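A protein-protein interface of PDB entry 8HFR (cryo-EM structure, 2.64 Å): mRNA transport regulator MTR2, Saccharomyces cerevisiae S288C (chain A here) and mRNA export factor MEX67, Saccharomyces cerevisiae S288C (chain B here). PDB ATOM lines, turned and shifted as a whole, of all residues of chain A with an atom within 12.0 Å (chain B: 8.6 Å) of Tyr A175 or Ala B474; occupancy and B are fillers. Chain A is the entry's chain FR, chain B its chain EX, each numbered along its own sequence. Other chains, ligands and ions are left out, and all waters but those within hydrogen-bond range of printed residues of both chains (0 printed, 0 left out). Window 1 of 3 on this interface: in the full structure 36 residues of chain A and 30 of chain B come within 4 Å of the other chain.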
ATOM      1  N   ASN A  55     -30.947   2.561  20.114  1.00  0.00           N
ATOM      2  CA  ASN A  55     -30.089   3.722  19.820  1.00  0.00           C
ATOM      3  C   ASN A  55     -28.774   3.684  20.594  1.00  0.00           C
ATOM      4  O   ASN A  55     -28.332   4.698  21.139  1.00  0.00           O
ATOM      5  CB  ASN A  55     -30.829   5.043  20.063  1.00  0.00           C
ATOM      6  N   ALA A  56     -28.166   2.490  20.641  1.00  0.00           N
ATOM      7  CA  ALA A  56     -26.854   2.226  21.252  1.00  0.00           C
ATOM      8  C   ALA A  56     -26.824   2.596  22.736  1.00  0.00           C
ATOM      9  O   ALA A  56     -25.916   3.280  23.213  1.00  0.00           O
ATOM     10  CB  ALA A  56     -25.727   2.922  20.483  1.00  0.00           C
ATOM     11  N   GLN A  77     -42.502   6.738  10.665  1.00  0.00           N
ATOM     12  CA  GLN A  77     -42.753   5.615   9.778  1.00  0.00           C
ATOM     13  C   GLN A  77     -41.416   4.989   9.418  1.00  0.00           C
ATOM     14  O   GLN A  77     -40.356   5.619   9.532  1.00  0.00           O
ATOM     15  CB  GLN A  77     -43.516   6.042   8.515  1.00  0.00           C
ATOM     16  N   ALA A  79     -39.209   1.693   7.005  1.00  0.00           N
ATOM     17  CA  ALA A  79     -39.099   0.784   5.873  1.00  0.00           C
ATOM     18  C   ALA A  79     -37.795   0.009   6.003  1.00  0.00           C
ATOM     19  O   ALA A  79     -36.894   0.399   6.749  1.00  0.00           O
ATOM     20  CB  ALA A  79     -39.148   1.527   4.533  1.00  0.00           C
ATOM     21  N   THR A  81     -34.326  -1.906   4.224  1.00  0.00           N
ATOM     22  CA  THR A  81     -33.377  -1.768   3.127  1.00  0.00           C
ATOM     23  C   THR A  81     -32.720  -3.088   2.765  1.00  0.00           C
ATOM     24  O   THR A  81     -32.609  -3.415   1.578  1.00  0.00           O
ATOM     25  CB  THR A  81     -32.306  -0.726   3.487  1.00  0.00           C
ATOM     26  N   VAL A  98     -30.870  -6.313  10.222  1.00  0.00           N
ATOM     27  CA  VAL A  98     -31.585  -5.602   9.179  1.00  0.00           C
ATOM     28  C   VAL A  98     -31.268  -4.117   9.257  1.00  0.00           C
ATOM     29  O   VAL A  98     -30.918  -3.587  10.318  1.00  0.00           O
ATOM     30  CB  VAL A  98     -33.101  -5.821   9.293  1.00  0.00           C
ATOM     31  N   ASN A  99     -31.374  -3.453   8.111  1.00  0.00           N
ATOM     32  CA  ASN A  99     -31.158  -2.017   7.994  1.00  0.00           C
ATOM     33  C   ASN A  99     -32.500  -1.324   7.791  1.00  0.00           C
ATOM     34  O   ASN A  99     -33.293  -1.735   6.933  1.00  0.00           O
ATOM     35  CB  ASN A  99     -30.203  -1.703   6.840  1.00  0.00           C
ATOM     36  N   CYS A 100     -32.754  -0.276   8.570  1.00  0.00           N
ATOM     37  CA  CYS A 100     -34.060   0.365   8.624  1.00  0.00           C
ATOM     38  C   CYS A 100     -33.944   1.827   8.229  1.00  0.00           C
ATOM     39  O   CYS A 100     -33.126   2.565   8.785  1.00  0.00           O
ATOM     40  CB  CYS A 100     -34.671   0.252  10.025  1.00  0.00           C
ATOM     41  N   LYS A 101     -34.765   2.244   7.275  1.00  0.00           N
ATOM     42  CA  LYS A 101     -34.977   3.656   7.016  1.00  0.00           C
ATOM     43  C   LYS A 101     -36.120   4.127   7.901  1.00  0.00           C
ATOM     44  O   LYS A 101     -37.149   3.452   8.002  1.00  0.00           O
ATOM     45  CB  LYS A 101     -35.298   3.903   5.542  1.00  0.00           C
ATOM     46  N   VAL A 102     -35.929   5.266   8.558  1.00  0.00           N
ATOM     47  CA  VAL A 102     -36.939   5.854   9.420  1.00  0.00           C
ATOM     48  C   VAL A 102     -37.165   7.302   9.014  1.00  0.00           C
ATOM     49  O   VAL A 102     -36.288   7.943   8.423  1.00  0.00           O
ATOM     50  CB  VAL A 102     -36.530   5.780  10.899  1.00  0.00           C
ATOM     51  N   ARG A 103     -38.363   7.801   9.321  1.00  0.00           N
ATOM     52  CA  ARG A 103     -38.673   9.212   9.103  1.00  0.00           C
ATOM     53  C   ARG A 103     -39.777   9.621  10.065  1.00  0.00           C
ATOM     54  O   ARG A 103     -40.849   9.014  10.067  1.00  0.00           O
ATOM     55  CB  ARG A 103     -39.093   9.480   7.653  1.00  0.00           C
ATOM     56  N   PHE A 104     -39.516  10.644  10.873  1.00  0.00           N
ATOM     57  CA  PHE A 104     -40.482  11.123  11.851  1.00  0.00           C
ATOM     58  C   PHE A 104     -41.179  12.384  11.353  1.00  0.00           C
ATOM     59  O   PHE A 104     -40.819  12.964  10.326  1.00  0.00           O
ATOM     60  CB  PHE A 104     -39.812  11.395  13.200  1.00  0.00           C
ATOM     61  N   GLY A 142     -39.932  13.733   6.524  1.00  0.00           N
ATOM     62  CA  GLY A 142     -38.698  14.452   6.780  1.00  0.00           C
ATOM     63  C   GLY A 142     -37.552  13.821   5.993  1.00  0.00           C
ATOM     64  O   GLY A 142     -37.757  12.982   5.111  1.00  0.00           O
ATOM     65  N   PRO A 143     -36.330  14.242   6.297  1.00  0.00           N
ATOM     66  CA  PRO A 143     -35.159  13.601   5.721  1.00  0.00           C
ATOM     67  C   PRO A 143     -34.992  12.218   6.330  1.00  0.00           C
ATOM     68  O   PRO A 143     -35.018  12.061   7.554  1.00  0.00           O
ATOM     69  CB  PRO A 143     -33.912  14.449   5.958  1.00  0.00           C
ATOM     70  N   TYR A 144     -34.842  11.214   5.469  1.00  0.00           N
ATOM     71  CA  TYR A 144     -34.804   9.830   5.923  1.00  0.00           C
ATOM     72  C   TYR A 144     -33.495   9.532   6.644  1.00  0.00           C
ATOM     73  O   TYR A 144     -32.406   9.799   6.127  1.00  0.00           O
ATOM     74  CB  TYR A 144     -34.986   8.882   4.740  1.00  0.00           C
ATOM     75  N   PHE A 145     -33.609   8.987   7.852  1.00  0.00           N
ATOM     76  CA  PHE A 145     -32.461   8.602   8.653  1.00  0.00           C
ATOM     77  C   PHE A 145     -32.363   7.082   8.673  1.00  0.00           C
ATOM     78  O   PHE A 145     -33.303   6.380   8.298  1.00  0.00           O
ATOM     79  CB  PHE A 145     -32.558   9.157  10.080  1.00  0.00           C
ATOM     80  N   GLY A 146     -31.217   6.570   9.108  1.00  0.00           N
ATOM     81  CA  GLY A 146     -30.940   5.145   9.019  1.00  0.00           C
ATOM     82  C   GLY A 146     -30.617   4.556  10.384  1.00  0.00           C
ATOM     83  O   GLY A 146     -29.979   5.198  11.223  1.00  0.00           O
ATOM     84  N   ILE A 147     -31.041   3.314  10.584  1.00  0.00           N
ATOM     85  CA  ILE A 147     -30.691   2.539  11.759  1.00  0.00           C
ATOM     86  C   ILE A 147     -30.303   1.136  11.318  1.00  0.00           C
ATOM     87  O   ILE A 147     -30.623   0.700  10.212  1.00  0.00           O
ATOM     88  CB  ILE A 147     -31.850   2.483  12.765  1.00  0.00           C
ATOM     89  N   SER A 148     -29.609   0.428  12.200  1.00  0.00           N
ATOM     90  CA  SER A 148     -29.324  -0.988  12.017  1.00  0.00           C
ATOM     91  C   SER A 148     -29.760  -1.734  13.269  1.00  0.00           C
ATOM     92  O   SER A 148     -29.340  -1.384  14.378  1.00  0.00           O
ATOM     93  CB  SER A 148     -27.840  -1.225  11.728  1.00  0.00           C
ATOM     94  N   LEU A 149     -30.611  -2.746  13.098  1.00  0.00           N
ATOM     95  CA  LEU A 149     -31.166  -3.499  14.215  1.00  0.00           C
ATOM     96  C   LEU A 149     -30.827  -4.973  14.045  1.00  0.00           C
ATOM     97  O   LEU A 149     -31.136  -5.572  13.011  1.00  0.00           O
ATOM     98  CB  LEU A 149     -32.682  -3.303  14.322  1.00  0.00           C
ATOM     99  N   TYR A 171     -30.534  -2.100  18.510  1.00  0.00           N
ATOM    100  CA  TYR A 171     -30.640  -1.158  17.408  1.00  0.00           C
ATOM    101  C   TYR A 171     -29.698   0.012  17.646  1.00  0.00           C
ATOM    102  O   TYR A 171     -29.548   0.474  18.783  1.00  0.00           O
ATOM    103  CB  TYR A 171     -32.075  -0.654  17.245  1.00  0.00           C
ATOM    104  N   ASN A 172     -29.066   0.480  16.572  1.00  0.00           N
ATOM    105  CA  ASN A 172     -28.211   1.661  16.604  1.00  0.00           C
ATOM    106  C   ASN A 172     -28.595   2.573  15.450  1.00  0.00           C
ATOM    107  O   ASN A 172     -28.578   2.148  14.291  1.00  0.00           O
ATOM    108  CB  ASN A 172     -26.733   1.278  16.518  1.00  0.00           C
ATOM    109  N   MET A 173     -28.960   3.813  15.768  1.00  0.00           N
ATOM    110  CA  MET A 173     -29.190   4.833  14.752  1.00  0.00           C
ATOM    111  C   MET A 173     -27.847   5.272  14.178  1.00  0.00           C
ATOM    112  O   MET A 173     -27.023   5.852  14.892  1.00  0.00           O
ATOM    113  CB  MET A 173     -29.947   6.014  15.350  1.00  0.00           C
ATOM    114  N   VAL A 174     -27.625   4.994  12.891  1.00  0.00           N
ATOM    115  CA  VAL A 174     -26.296   5.151  12.305  1.00  0.00           C
ATOM    116  C   VAL A 174     -26.012   6.602  11.924  1.00  0.00           C
ATOM    117  O   VAL A 174     -25.097   7.228  12.467  1.00  0.00           O
ATOM    118  CB  VAL A 174     -26.152   4.237  11.085  1.00  0.00           C
ATOM    119  N   TYR A 175     -26.791   7.151  10.992  1.00  0.00           N
ATOM    120  CA  TYR A 175     -26.574   8.496  10.483  1.00  0.00           C
ATOM    121  C   TYR A 175     -27.910   9.155  10.173  1.00  0.00           C
ATOM    122  O   TYR A 175     -28.967   8.515  10.190  1.00  0.00           O
ATOM    123  CB  TYR A 175     -25.696   8.495   9.227  1.00  0.00           C
ATOM    124  N   LYS A 176     -27.841  10.450   9.874  1.00  0.00           N
ATOM    125  CA  LYS A 176     -29.004  11.237   9.491  1.00  0.00           C
ATOM    126  C   LYS A 176     -28.524  12.440   8.694  1.00  0.00           C
ATOM    127  O   LYS A 176     -27.324  12.634   8.484  1.00  0.00           O
ATOM    128  CB  LYS A 176     -29.819  11.681  10.709  1.00  0.00           C
ATOM    129  N   PRO A 177     -29.480  13.241   8.242  1.00  0.00           N
ATOM    130  CA  PRO A 177     -29.181  14.463   7.517  1.00  0.00           C
ATOM    131  C   PRO A 177     -29.136  15.642   8.489  1.00  0.00           C
ATOM    132  O   PRO A 177     -29.135  15.474   9.710  1.00  0.00           O
ATOM    133  CB  PRO A 177     -30.202  14.682   6.404  1.00  0.00           C
ATOM    134  N   GLU A 178     -29.101  16.856   7.944  1.00  0.00           N
ATOM    135  CA  GLU A 178     -29.150  18.067   8.746  1.00  0.00           C
ATOM    136  C   GLU A 178     -30.536  18.690   8.813  1.00  0.00           C
ATOM    137  O   GLU A 178     -30.805  19.463   9.738  1.00  0.00           O
ATOM    138  CB  GLU A 178     -28.164  19.105   8.201  1.00  0.00           C
ATOM    139  N   ASP A 179     -31.418  18.369   7.866  1.00  0.00           N
ATOM    140  CA  ASP A 179     -32.710  19.028   7.737  1.00  0.00           C
ATOM    141  C   ASP A 179     -33.840  18.221   8.361  1.00  0.00           C
ATOM    142  O   ASP A 179     -34.970  18.246   7.865  1.00  0.00           O
ATOM    143  CB  ASP A 179     -33.010  19.319   6.267  1.00  0.00           C
ATOM    144  N   SER A 180     -33.553  17.501   9.437  1.00  0.00           N
ATOM    145  CA  SER A 180     -34.581  16.862  10.242  1.00  0.00           C
ATOM    146  C   SER A 180     -34.988  17.811  11.369  1.00  0.00           C
ATOM    147  O   SER A 180     -34.606  18.985  11.394  1.00  0.00           O
ATOM    148  CB  SER A 180     -34.083  15.523  10.778  1.00  0.00           C
ATOM    149  N   LEU A 181     -35.776  17.308  12.315  1.00  0.00           N
ATOM    150  CA  LEU A 181     -36.115  18.074  13.507  1.00  0.00           C
ATOM    151  C   LEU A 181     -35.831  17.235  14.742  1.00  0.00           C
ATOM    152  O   LEU A 181     -35.549  17.772  15.819  1.00  0.00           O
ATOM    153  CB  LEU A 181     -37.579  18.513  13.478  1.00  0.00           C
ATOM    154  N   LEU A 182     -35.904  15.914  14.584  1.00  0.00           N
ATOM    155  CA  LEU A 182     -35.650  14.991  15.681  1.00  0.00           C
ATOM    156  C   LEU A 182     -34.168  14.973  16.027  1.00  0.00           C
ATOM    157  O   LEU A 182     -33.330  14.607  15.198  1.00  0.00           O
ATOM    158  CB  LEU A 182     -36.126  13.589  15.308  1.00  0.00           C
ATOM    159  N   LYS A 183     -33.846  15.363  17.258  1.00  0.00           N
ATOM    160  CA  LYS A 183     -32.470  15.462  17.724  1.00  0.00           C
ATOM    161  C   LYS A 183     -32.148  14.258  18.600  1.00  0.00           C
ATOM    162  O   LYS A 183     -32.725  14.098  19.682  1.00  0.00           O
ATOM    163  CB  LYS A 183     -32.244  16.765  18.493  1.00  0.00           C
ATOM    164  N   ILE A 184     -31.231  13.420  18.127  1.00  0.00           N
ATOM    165  CA  ILE A 184     -30.762  12.265  18.886  1.00  0.00           C
ATOM    166  C   ILE A 184     -29.348  11.891  18.453  1.00  0.00           C
ATOM    167  O   ILE A 184     -28.582  12.742  18.004  1.00  0.00           O
ATOM    168  CB  ILE A 184     -31.706  11.081  18.708  1.00  0.00           C
ATOM    169  N   ILE B 267     -29.016   9.757  22.732  1.00  0.00           N
ATOM    170  CA  ILE B 267     -28.118   8.859  22.014  1.00  0.00           C
ATOM    171  C   ILE B 267     -26.834   8.750  22.824  1.00  0.00           C
ATOM    172  O   ILE B 267     -26.063   9.710  22.920  1.00  0.00           O
ATOM    173  CB  ILE B 267     -27.855   9.365  20.601  1.00  0.00           C
ATOM    174  N   GLN B 268     -26.618   7.582  23.425  1.00  0.00           N
ATOM    175  CA  GLN B 268     -25.412   7.348  24.207  1.00  0.00           C
ATOM    176  C   GLN B 268     -24.203   7.283  23.284  1.00  0.00           C
ATOM    177  O   GLN B 268     -24.248   6.630  22.237  1.00  0.00           O
ATOM    178  CB  GLN B 268     -25.543   6.057  25.013  1.00  0.00           C
ATOM    179  N   ILE B 317     -29.243   4.558   0.489  1.00  0.00           N
ATOM    180  CA  ILE B 317     -28.355   5.538   1.103  1.00  0.00           C
ATOM    181  C   ILE B 317     -29.198   6.479   1.953  1.00  0.00           C
ATOM    182  O   ILE B 317     -30.393   6.252   2.164  1.00  0.00           O
ATOM    183  CB  ILE B 317     -27.550   6.299   0.047  1.00  0.00           C
ATOM    184  N   PRO B 318     -28.568   7.547   2.434  1.00  0.00           N
ATOM    185  CA  PRO B 318     -29.199   8.520   3.311  1.00  0.00           C
ATOM    186  C   PRO B 318     -29.813   9.650   2.483  1.00  0.00           C
ATOM    187  O   PRO B 318     -29.978   9.544   1.265  1.00  0.00           O
ATOM    188  CB  PRO B 318     -28.187   9.043   4.325  1.00  0.00           C
ATOM    189  N   PRO B 319     -30.168  10.741   3.154  1.00  0.00           N
ATOM    190  CA  PRO B 319     -30.790  11.896   2.520  1.00  0.00           C
ATOM    191  C   PRO B 319     -29.724  12.801   1.902  1.00  0.00           C
ATOM    192  O   PRO B 319     -28.562  12.421   1.733  1.00  0.00           O
ATOM    193  CB  PRO B 319     -31.652  12.649   3.527  1.00  0.00           C
ATOM    194  N   VAL B 322     -27.018  14.974   4.515  1.00  0.00           N
ATOM    195  CA  VAL B 322     -26.166  14.151   5.368  1.00  0.00           C
ATOM    196  C   VAL B 322     -24.702  14.434   5.061  1.00  0.00           C
ATOM    197  O   VAL B 322     -24.207  14.091   3.981  1.00  0.00           O
ATOM    198  CB  VAL B 322     -26.498  12.676   5.165  1.00  0.00           C
ATOM    199  N   THR B 323     -24.009  15.061   6.006  1.00  0.00           N
ATOM    200  CA  THR B 323     -22.595  15.358   5.834  1.00  0.00           C
ATOM    201  C   THR B 323     -21.751  14.114   6.089  1.00  0.00           C
ATOM    202  O   THR B 323     -22.128  13.235   6.871  1.00  0.00           O
ATOM    203  CB  THR B 323     -22.167  16.484   6.772  1.00  0.00           C
ATOM    204  N   ASP B 324     -20.599  14.058   5.405  1.00  0.00           N
ATOM    205  CA  ASP B 324     -19.691  12.901   5.354  1.00  0.00           C
ATOM    206  C   ASP B 324     -20.395  11.624   4.896  1.00  0.00           C
ATOM    207  O   ASP B 324     -20.036  10.522   5.314  1.00  0.00           O
ATOM    208  CB  ASP B 324     -18.975  12.666   6.692  1.00  0.00           C
ATOM    209  N   SER B 325     -21.385  11.758   4.020  1.00  0.00           N
ATOM    210  CA  SER B 325     -22.116  10.621   3.486  1.00  0.00           C
ATOM    211  C   SER B 325     -21.686  10.344   2.050  1.00  0.00           C
ATOM    212  O   SER B 325     -21.307  11.254   1.308  1.00  0.00           O
ATOM    213  CB  SER B 325     -23.625  10.863   3.543  1.00  0.00           C
ATOM    214  N   ASP B 326     -21.746   9.069   1.666  1.00  0.00           N
ATOM    215  CA  ASP B 326     -21.334   8.617   0.336  1.00  0.00           C
ATOM    216  C   ASP B 326     -22.478   7.813  -0.276  1.00  0.00           C
ATOM    217  O   ASP B 326     -22.577   6.600  -0.077  1.00  0.00           O
ATOM    218  CB  ASP B 326     -20.044   7.810   0.409  1.00  0.00           C
ATOM    219  N   GLU B 381     -16.365   7.078  17.318  1.00  0.00           N
ATOM    220  CA  GLU B 381     -17.402   6.800  16.337  1.00  0.00           C
ATOM    221  C   GLU B 381     -17.786   5.331  16.266  1.00  0.00           C
ATOM    222  O   GLU B 381     -18.880   5.021  15.783  1.00  0.00           O
ATOM    223  CB  GLU B 381     -16.969   7.271  14.939  1.00  0.00           C
ATOM    224  N   SER B 444     -18.763   1.884   5.161  1.00  0.00           N
ATOM    225  CA  SER B 444     -19.313   1.898   6.516  1.00  0.00           C
ATOM    226  C   SER B 444     -19.886   0.521   6.831  1.00  0.00           C
ATOM    227  O   SER B 444     -20.951   0.144   6.335  1.00  0.00           O
ATOM    228  CB  SER B 444     -20.373   2.980   6.666  1.00  0.00           C
ATOM    229  N   ALA B 469     -24.004   2.684   3.001  1.00  0.00           N
ATOM    230  CA  ALA B 469     -23.376   3.901   2.499  1.00  0.00           C
ATOM    231  C   ALA B 469     -22.406   4.472   3.527  1.00  0.00           C
ATOM    232  O   ALA B 469     -22.682   4.479   4.730  1.00  0.00           O
ATOM    233  CB  ALA B 469     -24.444   4.941   2.156  1.00  0.00           C
ATOM    234  N   TYR B 470     -21.259   4.954   3.041  1.00  0.00           N
ATOM    235  CA  TYR B 470     -20.191   5.455   3.908  1.00  0.00           C
ATOM    236  C   TYR B 470     -20.602   6.812   4.462  1.00  0.00           C
ATOM    237  O   TYR B 470     -20.231   7.874   3.956  1.00  0.00           O
ATOM    238  CB  TYR B 470     -18.874   5.536   3.155  1.00  0.00           C
ATOM    239  N   SER B 471     -21.384   6.764   5.536  1.00  0.00           N
ATOM    240  CA  SER B 471     -21.945   7.947   6.168  1.00  0.00           C
ATOM    241  C   SER B 471     -21.334   8.149   7.548  1.00  0.00           C
ATOM    242  O   SER B 471     -20.622   7.294   8.076  1.00  0.00           O
ATOM    243  CB  SER B 471     -23.471   7.838   6.265  1.00  0.00           C
ATOM    244  N   THR B 472     -21.637   9.312   8.124  1.00  0.00           N
ATOM    245  CA  THR B 472     -21.091   9.747   9.401  1.00  0.00           C
ATOM    246  C   THR B 472     -21.903   9.148  10.547  1.00  0.00           C
ATOM    247  O   THR B 472     -22.643   8.175  10.381  1.00  0.00           O
ATOM    248  CB  THR B 472     -21.056  11.270   9.465  1.00  0.00           C
ATOM    249  N   GLY B 473     -21.733   9.699  11.748  1.00  0.00           N
ATOM    250  CA  GLY B 473     -22.496   9.293  12.921  1.00  0.00           C
ATOM    251  C   GLY B 473     -23.366  10.465  13.365  1.00  0.00           C
ATOM    252  O   GLY B 473     -22.848  11.509  13.776  1.00  0.00           O
ATOM    253  N   ALA B 474     -24.688  10.291  13.274  1.00  0.00           N
ATOM    254  CA  ALA B 474     -25.605  11.337  13.719  1.00  0.00           C
ATOM    255  C   ALA B 474     -25.777  11.326  15.227  1.00  0.00           C
ATOM    256  O   ALA B 474     -26.216  12.328  15.804  1.00  0.00           O
ATOM    257  CB  ALA B 474     -26.964  11.181  13.048  1.00  0.00           C
ATOM    258  N   TRP B 475     -25.458  10.203  15.877  1.00  0.00           N
ATOM    259  CA  TRP B 475     -25.430  10.158  17.332  1.00  0.00           C
ATOM    260  C   TRP B 475     -24.309  11.017  17.899  1.00  0.00           C
ATOM    261  O   TRP B 475     -24.408  11.472  19.044  1.00  0.00           O
ATOM    262  CB  TRP B 475     -25.282   8.715  17.811  1.00  0.00           C
ATOM    263  N   LYS B 476     -23.251  11.243  17.124  1.00  0.00           N
ATOM    264  CA  LYS B 476     -22.206  12.171  17.508  1.00  0.00           C
ATOM    265  C   LYS B 476     -22.706  13.610  17.379  1.00  0.00           C
ATOM    266  O   LYS B 476     -23.745  13.888  16.773  1.00  0.00           O
ATOM    267  CB  LYS B 476     -20.958  11.950  16.654  1.00  0.00           C
ATOM    268  N   THR B 477     -21.946  14.531  17.959  1.00  0.00           N
ATOM    269  CA  THR B 477     -22.369  15.922  18.051  1.00  0.00           C
ATOM    270  C   THR B 477     -21.172  16.855  18.190  1.00  0.00           C
ATOM    271  O   THR B 477     -21.177  17.764  19.019  1.00  0.00           O
ATOM    272  CB  THR B 477     -23.323  16.106  19.224  1.00  0.00           C
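N of Ala B474 lies within hydrogen-bond range of O of Val A174 (3.2 Å). O of Val A174 sits close to O of Thr B472, at 3.4 Å. The backbone carbonyl oxygen (O) of Ala B474 lies close to the backbone carbonyl oxygen (O) of Ile A184, at 3.3 Å.
Printed residues of chain B within 4 Å of Ala A56: Gln B268 (3.3 Å). Printed residues of chain B within 4 Å of Pro A143: Pro B319. Tyr A175 touches three residues of chain B. Of chain B, only Val B322 (3.4 Å) and Ala B474 (3.4 Å) come within 4 Å of Lys A176. Printed residues of chain B within 4 Å of Ile A184: Ile B267 (3.6 Å) and Ala B474 (3.3 Å). Of the printed residues of chain A, Pro B319 touches Pro A143, Tyr A144 and Pro A177. Of the printed residues of chain A, Val B322 touches Lys A176 and Pro A177. Printed residues of chain A within 4 Å of Ser B471: Tyr A175. Of chain A, only Val A174 (3.4 Å) and Tyr A175 (3.3 Å) come within 4 Å of Thr B472. Gly B473 touches just one residue of chain A: Val A174 (3.4 Å). Of chain A, only Val A174 (3.2 Å), Tyr A175 (3.6 Å), Lys A176 (3.4 Å) and Ile A184 (3.3 Å) come within 4 Å of Ala B474. No residue of chain A comes within 4 Å of Lys B476.
The backbone carbonyl oxygen (O) of Tyr A171 is in hydrogen-bond range of the backbone NH (N) of Ala A56 (3.1 Å). The backbone NH (N) of Val A174 lies within hydrogen-bond range of the backbone carbonyl oxygen (O) of Gly A146. N of Thr B472 lies within hydrogen-bond range of O of Asp B324, 3.5 Å away. N of Gly A146 lies within hydrogen-bond range of O of Tyr A175 (3.2 Å).
Ala A56 touches Gln B268. Pro A143 touches Pro B319 (CB to CB, 3.8 Å). O of Tyr A144 touches N of Pro B319, at 3.8 Å. Val A174 touches Gly B473. Ser B471 touches Tyr A175. CB of Tyr A175 touches O of Thr B472, at 3.3 Å. O of Lys A176 touches CB of Val B322 (3.4 Å). Lys A176 touches Ala B474 (N to CB, 3.4 Å). CB of Pro A177 touches N of Val B322 (3.7 Å). Ile A184 touches Ile B267 (C to CB, 3.6 Å).
Of the 21 printed residues of chain B, 8 touch a printed residue of chain A. Printed residues of chain B that touch a printed residue of chain A: Ile B267, Gln B268, Pro B319, Val B322, Ser B471, Thr B472, Gly B473 and Ala B474. Hydrophobic or aromatic side chains of chain B that line the printed part of chain A: Ile B267, Pro B319, Val B322 and Ala B474. Along chain B the printed residues that touch a printed residue of chain A span positions 267 to 474. Of the 34 printed residues of chain A, 8 touch a printed residue of chain B. Printed residues of chain A that touch a printed residue of chain B: Ala A56, Pro A143, Tyr A144, Val A174, Tyr A175, Lys A176, Pro A177 and Ile A184.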
